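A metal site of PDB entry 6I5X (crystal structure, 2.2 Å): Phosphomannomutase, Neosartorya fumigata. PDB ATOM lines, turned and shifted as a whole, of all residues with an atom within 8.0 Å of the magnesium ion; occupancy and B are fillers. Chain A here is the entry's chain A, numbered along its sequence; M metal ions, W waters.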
ATOM      1  N   PHE A  16      -8.687  -6.337  -0.566  1.00  0.00           N
ATOM      2  CA  PHE A  16      -9.562  -7.417  -1.006  1.00  0.00           C
ATOM      3  C   PHE A  16     -10.811  -7.497  -0.167  1.00  0.00           C
ATOM      4  O   PHE A  16     -10.744  -7.483   1.064  1.00  0.00           O
ATOM      5  CB  PHE A  16      -8.840  -8.744  -0.949  1.00  0.00           C
ATOM      6  CG  PHE A  16      -7.567  -8.798  -1.757  1.00  0.00           C
ATOM      7  CD1 PHE A  16      -6.354  -8.396  -1.204  1.00  0.00           C
ATOM      8  CD2 PHE A  16      -7.580  -9.287  -3.046  1.00  0.00           C
ATOM      9  CE1 PHE A  16      -5.181  -8.470  -1.928  1.00  0.00           C
ATOM     10  CE2 PHE A  16      -6.416  -9.371  -3.788  1.00  0.00           C
ATOM     11  CZ  PHE A  16      -5.192  -8.954  -3.226  1.00  0.00           C
ATOM     12  N   ASP A  17     -11.945  -7.614  -0.829  1.00  0.00           N
ATOM     13  CA  ASP A  17     -13.147  -8.181  -0.223  1.00  0.00           C
ATOM     14  C   ASP A  17     -12.822  -9.604   0.242  1.00  0.00           C
ATOM     15  O   ASP A  17     -11.868 -10.202  -0.244  1.00  0.00           O
ATOM     16  CB  ASP A  17     -14.288  -8.151  -1.231  1.00  0.00           C
ATOM     17  CG  ASP A  17     -15.531  -8.926  -0.732  1.00  0.00           C
ATOM     18  OD1 ASP A  17     -16.037  -8.584   0.357  1.00  0.00           O
ATOM     19  OD2 ASP A  17     -15.983  -9.862  -1.440  1.00  0.00           O
ATOM     20  N   VAL A  18     -13.533 -10.122   1.243  1.00  0.00           N
ATOM     21  CA  VAL A  18     -13.268 -11.490   1.711  1.00  0.00           C
ATOM     22  C   VAL A  18     -14.184 -12.506   0.990  1.00  0.00           C
ATOM     23  O   VAL A  18     -13.698 -13.311   0.161  1.00  0.00           O
ATOM     24  CB  VAL A  18     -13.358 -11.607   3.255  1.00  0.00           C
ATOM     25  CG1 VAL A  18     -12.920 -12.997   3.688  1.00  0.00           C
ATOM     26  CG2 VAL A  18     -12.457 -10.565   3.907  1.00  0.00           C
ATOM     27  N   ASP A  19     -15.478 -12.483   1.308  1.00  0.00           N
ATOM     28  CA  ASP A  19     -16.387 -13.557   0.853  1.00  0.00           C
ATOM     29  C   ASP A  19     -16.583 -13.550  -0.663  1.00  0.00           C
ATOM     30  O   ASP A  19     -17.017 -12.565  -1.231  1.00  0.00           O
ATOM     31  CB  ASP A  19     -17.755 -13.483   1.562  1.00  0.00           C
ATOM     32  CG  ASP A  19     -17.704 -13.913   2.995  1.00  0.00           C
ATOM     33  OD1 ASP A  19     -17.018 -14.921   3.298  1.00  0.00           O
ATOM     34  OD2 ASP A  19     -18.344 -13.221   3.854  1.00  0.00           O
ATOM     35  N   GLU A  20     -16.227 -14.665  -1.281  1.00  0.00           N
ATOM     36  CA  GLU A  20     -16.224 -14.881  -2.719  1.00  0.00           C
ATOM     37  C   GLU A  20     -15.214 -14.044  -3.491  1.00  0.00           C
ATOM     38  O   GLU A  20     -15.335 -13.888  -4.708  1.00  0.00           O
ATOM     39  CB  GLU A  20     -17.651 -14.709  -3.298  1.00  0.00           C
ATOM     40  CG  GLU A  20     -18.542 -15.861  -2.810  1.00  0.00           C
ATOM     41  CD  GLU A  20     -18.097 -17.173  -3.506  1.00  0.00           C
ATOM     42  OE1 GLU A  20     -17.623 -17.184  -4.668  1.00  0.00           O
ATOM     43  OE2 GLU A  20     -18.129 -18.205  -2.845  1.00  0.00           O
ATOM     44  N   THR A  21     -14.204 -13.539  -2.792  1.00  0.00           N
ATOM     45  CA  THR A  21     -13.096 -12.836  -3.418  1.00  0.00           C
ATOM     46  C   THR A  21     -11.791 -13.528  -2.996  1.00  0.00           C
ATOM     47  O   THR A  21     -11.045 -14.007  -3.857  1.00  0.00           O
ATOM     48  CB  THR A  21     -13.117 -11.348  -3.043  1.00  0.00           C
ATOM     49  OG1 THR A  21     -14.277 -10.731  -3.630  1.00  0.00           O
ATOM     50  CG2 THR A  21     -11.860 -10.625  -3.542  1.00  0.00           C
ATOM     51  N   LEU A  22     -11.533 -13.570  -1.677  1.00  0.00           N
ATOM     52  CA  LEU A  22     -10.431 -14.338  -1.138  1.00  0.00           C
ATOM     53  C   LEU A  22     -10.769 -15.806  -0.820  1.00  0.00           C
ATOM     54  O   LEU A  22      -9.890 -16.690  -0.883  1.00  0.00           O
ATOM     55  CB  LEU A  22      -9.883 -13.692   0.135  1.00  0.00           C
ATOM     56  CG  LEU A  22      -9.247 -12.312  -0.034  1.00  0.00           C
ATOM     57  CD1 LEU A  22      -8.684 -11.817   1.283  1.00  0.00           C
ATOM     58  CD2 LEU A  22      -8.164 -12.350  -1.094  1.00  0.00           C
ATOM     59  N   THR A  23     -12.016 -16.054  -0.431  1.00  0.00           N
ATOM     60  CA  THR A  23     -12.456 -17.380   0.048  1.00  0.00           C
ATOM     61  C   THR A  23     -13.816 -17.691  -0.523  1.00  0.00           C
ATOM     62  O   THR A  23     -14.573 -16.754  -0.827  1.00  0.00           O
ATOM     63  CB  THR A  23     -12.702 -17.347   1.578  1.00  0.00           C
ATOM     64  OG1 THR A  23     -13.834 -16.492   1.882  1.00  0.00           O
ATOM     65  CG2 THR A  23     -11.516 -16.872   2.295  1.00  0.00           C
ATOM     66  N   ALA A  25     -17.695 -18.181   0.031  1.00  0.00           N
ATOM     67  CA  ALA A  25     -18.510 -17.448   1.012  1.00  0.00           C
ATOM     68  C   ALA A  25     -18.575 -18.247   2.304  1.00  0.00           C
ATOM     69  O   ALA A  25     -18.983 -19.355   2.275  1.00  0.00           O
ATOM     70  CB  ALA A  25     -19.930 -17.146   0.484  1.00  0.00           C
ATOM     71  N   VAL A  49     -10.982  -5.921   3.365  1.00  0.00           N
ATOM     72  CA  VAL A  49     -12.107  -5.173   3.901  1.00  0.00           C
ATOM     73  C   VAL A  49     -13.360  -6.014   3.705  1.00  0.00           C
ATOM     74  O   VAL A  49     -13.698  -6.426   2.593  1.00  0.00           O
ATOM     75  CB  VAL A  49     -12.246  -3.734   3.300  1.00  0.00           C
ATOM     76  CG1 VAL A  49     -12.304  -3.754   1.775  1.00  0.00           C
ATOM     77  CG2 VAL A  49     -13.476  -3.023   3.866  1.00  0.00           C
ATOM     78  N   GLY A  50     -14.052  -6.304   4.807  1.00  0.00           N
ATOM     79  CA  GLY A  50     -15.221  -7.173   4.760  1.00  0.00           C
ATOM     80  C   GLY A  50     -16.273  -6.686   5.725  1.00  0.00           C
ATOM     81  O   GLY A  50     -15.976  -5.957   6.665  1.00  0.00           O
ATOM     82  N   GLY A  51     -17.530  -7.042   5.443  1.00  0.00           N
ATOM     83  CA  GLY A  51     -18.658  -6.607   6.268  1.00  0.00           C
ATOM     84  C   GLY A  51     -18.690  -7.245   7.643  1.00  0.00           C
ATOM     85  O   GLY A  51     -19.089  -6.583   8.578  1.00  0.00           O
ATOM     86  N   LYS A 197     -17.979   0.044   2.342  1.00  0.00           N
ATOM     87  CA  LYS A 197     -16.548  -0.336   2.307  1.00  0.00           C
ATOM     88  C   LYS A 197     -15.577   0.839   2.047  1.00  0.00           C
ATOM     89  O   LYS A 197     -14.405   0.754   2.429  1.00  0.00           O
ATOM     90  CB  LYS A 197     -16.317  -1.413   1.256  1.00  0.00           C
ATOM     91  CG  LYS A 197     -16.929  -2.749   1.664  1.00  0.00           C
ATOM     92  CD  LYS A 197     -16.365  -3.825   0.777  1.00  0.00           C
ATOM     93  CE  LYS A 197     -16.541  -5.212   1.378  1.00  0.00           C
ATOM     94  NZ  LYS A 197     -17.437  -6.161   0.659  1.00  0.00           N
ATOM     95  N   PHE A 220      -8.510  -2.493  -5.658  1.00  0.00           N
ATOM     96  CA  PHE A 220      -9.579  -3.125  -4.901  1.00  0.00           C
ATOM     97  C   PHE A 220     -10.128  -4.303  -5.686  1.00  0.00           C
ATOM     98  O   PHE A 220     -10.414  -4.151  -6.858  1.00  0.00           O
ATOM     99  CB  PHE A 220     -10.727  -2.175  -4.644  1.00  0.00           C
ATOM    100  CG  PHE A 220     -11.915  -2.879  -4.079  1.00  0.00           C
ATOM    101  CD1 PHE A 220     -11.921  -3.272  -2.728  1.00  0.00           C
ATOM    102  CD2 PHE A 220     -12.923  -3.306  -4.885  1.00  0.00           C
ATOM    103  CE1 PHE A 220     -12.993  -4.005  -2.233  1.00  0.00           C
ATOM    104  CE2 PHE A 220     -13.997  -4.005  -4.397  1.00  0.00           C
ATOM    105  CZ  PHE A 220     -14.028  -4.376  -3.075  1.00  0.00           C
ATOM    106  N   PHE A 221     -10.339  -5.425  -5.023  1.00  0.00           N
ATOM    107  CA  PHE A 221     -10.913  -6.624  -5.609  1.00  0.00           C
ATOM    108  C   PHE A 221     -12.164  -7.018  -4.864  1.00  0.00           C
ATOM    109  O   PHE A 221     -12.161  -7.096  -3.654  1.00  0.00           O
ATOM    110  CB  PHE A 221      -9.940  -7.816  -5.509  1.00  0.00           C
ATOM    111  CG  PHE A 221      -8.682  -7.641  -6.289  1.00  0.00           C
ATOM    112  CD1 PHE A 221      -7.679  -6.832  -5.808  1.00  0.00           C
ATOM    113  CD2 PHE A 221      -8.503  -8.293  -7.496  1.00  0.00           C
ATOM    114  CE1 PHE A 221      -6.494  -6.677  -6.488  1.00  0.00           C
ATOM    115  CE2 PHE A 221      -7.320  -8.116  -8.212  1.00  0.00           C
ATOM    116  CZ  PHE A 221      -6.321  -7.337  -7.700  1.00  0.00           C
ATOM    117  N   GLY A 222     -13.224  -7.281  -5.603  1.00  0.00           N
ATOM    118  CA  GLY A 222     -14.526  -7.610  -5.038  1.00  0.00           C
ATOM    119  C   GLY A 222     -15.391  -8.292  -6.051  1.00  0.00           C
ATOM    120  O   GLY A 222     -15.201  -8.159  -7.265  1.00  0.00           O
ATOM    121  N   ASP A 223     -16.361  -9.038  -5.543  1.00  0.00           N
ATOM    122  CA  ASP A 223     -17.288  -9.791  -6.388  1.00  0.00           C
ATOM    123  C   ASP A 223     -18.667  -9.156  -6.514  1.00  0.00           C
ATOM    124  O   ASP A 223     -19.430  -9.636  -7.300  1.00  0.00           O
ATOM    125  CB  ASP A 223     -17.401 -11.246  -5.887  1.00  0.00           C
ATOM    126  CG  ASP A 223     -18.081 -11.334  -4.496  1.00  0.00           C
ATOM    127  OD1 ASP A 223     -17.542 -10.759  -3.505  1.00  0.00           O
ATOM    128  OD2 ASP A 223     -19.167 -11.957  -4.412  1.00  0.00           O
ATOM    129  N   LYS A 224     -18.977  -8.109  -5.751  1.00  0.00           N
ATOM    130  CA  LYS A 224     -20.304  -7.438  -5.839  1.00  0.00           C
ATOM    131  C   LYS A 224     -20.131  -5.974  -6.201  1.00  0.00           C
ATOM    132  O   LYS A 224     -20.513  -5.067  -5.462  1.00  0.00           O
ATOM    133  CB  LYS A 224     -21.054  -7.583  -4.522  1.00  0.00           C
ATOM    134  CG  LYS A 224     -21.330  -9.000  -4.067  1.00  0.00           C
ATOM    135  CD  LYS A 224     -22.282  -9.694  -5.046  1.00  0.00           C
ATOM    136  CE  LYS A 224     -22.575 -11.134  -4.807  1.00  0.00           C
ATOM    137  NZ  LYS A 224     -23.915 -11.357  -4.233  1.00  0.00           N
ATOM    138  N   CYS A 225     -19.537  -5.764  -7.371  1.00  0.00           N
ATOM    139  CA  CYS A 225     -19.125  -4.426  -7.860  1.00  0.00           C
ATOM    140  C   CYS A 225     -20.176  -3.687  -8.707  1.00  0.00           C
ATOM    141  O   CYS A 225     -19.917  -2.585  -9.169  1.00  0.00           O
ATOM    142  CB  CYS A 225     -17.870  -4.575  -8.694  1.00  0.00           C
ATOM    143  SG  CYS A 225     -16.504  -5.236  -7.763  1.00  0.00           S
ATOM    144  N   ASN A 230     -22.380  -4.710  -2.332  1.00  0.00           N
ATOM    145  CA  ASN A 230     -21.600  -3.977  -1.299  1.00  0.00           C
ATOM    146  C   ASN A 230     -20.137  -3.646  -1.653  1.00  0.00           C
ATOM    147  O   ASN A 230     -19.450  -2.971  -0.868  1.00  0.00           O
ATOM    148  CB  ASN A 230     -21.754  -4.551   0.117  1.00  0.00           C
ATOM    149  CG  ASN A 230     -21.475  -5.993   0.216  1.00  0.00           C
ATOM    150  OD1 ASN A 230     -20.712  -6.547  -0.588  1.00  0.00           O
ATOM    151  ND2 ASN A 230     -22.090  -6.661   1.232  1.00  0.00           N
ATOM    152  N   ASP A 231     -19.683  -4.030  -2.839  1.00  0.00           N
ATOM    153  CA  ASP A 231     -18.391  -3.549  -3.322  1.00  0.00           C
ATOM    154  C   ASP A 231     -18.537  -2.396  -4.307  1.00  0.00           C
ATOM    155  O   ASP A 231     -17.537  -1.921  -4.792  1.00  0.00           O
ATOM    156  CB  ASP A 231     -17.595  -4.708  -3.946  1.00  0.00           C
ATOM    157  CG  ASP A 231     -17.436  -5.869  -3.008  1.00  0.00           C
ATOM    158  OD1 ASP A 231     -17.105  -5.623  -1.841  1.00  0.00           O
ATOM    159  OD2 ASP A 231     -17.649  -7.042  -3.436  1.00  0.00           O
ATOM    160  N   VAL A 245     -14.410  -9.556  -9.665  1.00  0.00           N
ATOM    161  CA  VAL A 245     -14.102 -10.985  -9.689  1.00  0.00           C
ATOM    162  C   VAL A 245     -15.357 -11.850  -9.572  1.00  0.00           C
ATOM    163  O   VAL A 245     -16.299 -11.458  -8.968  1.00  0.00           O
ATOM    164  CB  VAL A 245     -13.078 -11.393  -8.579  1.00  0.00           C
ATOM    165  CG1 VAL A 245     -11.816 -10.522  -8.670  1.00  0.00           C
ATOM    166  CG2 VAL A 245     -13.681 -11.329  -7.191  1.00  0.00           C
HETATM  167 MG    MG M   1     -17.963 -10.583  -1.435  1.00  0.00          MG
HETATM  168  O   HOH W   1     -18.060 -10.120   0.753  1.00  0.00           O
HETATM  169  O   HOH W   2     -18.489  -8.776  -1.878  1.00  0.00           O
HETATM  170  O   HOH W   3     -19.657 -11.573  -1.964  1.00  0.00           O
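OG1 of Thr 21 sits close to OD2 of Asp 17 (2.9 Å). NZ of Lys 197 lies within salt-bridge range of OD1 of Asp 17, 2.8 Å away. OG1 of Thr 21 is in hydrogen-bond range of N of Asp 223 (3.3 Å). The backbone NH (N) of Asp 17 lies within hydrogen-bond range of the backbone carbonyl oxygen (O) of Phe 221, 2.9 Å away. OD2 of Asp 231 sits at hydrogen-bond distance from N of Asp 223 (3.2 Å).
Within 4 Å of the magnesium ion: Asp 17, Asp 19 and Asp 223.
The magnesium ion is bound by water W2 (1.9 Å), water W3 (2.0 Å), OD2 of Asp 17 (2.1 Å), OD1 of Asp 223 (2.1 Å), O of Asp 19 (2.2 Å) and water W1 (2.2 Å).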
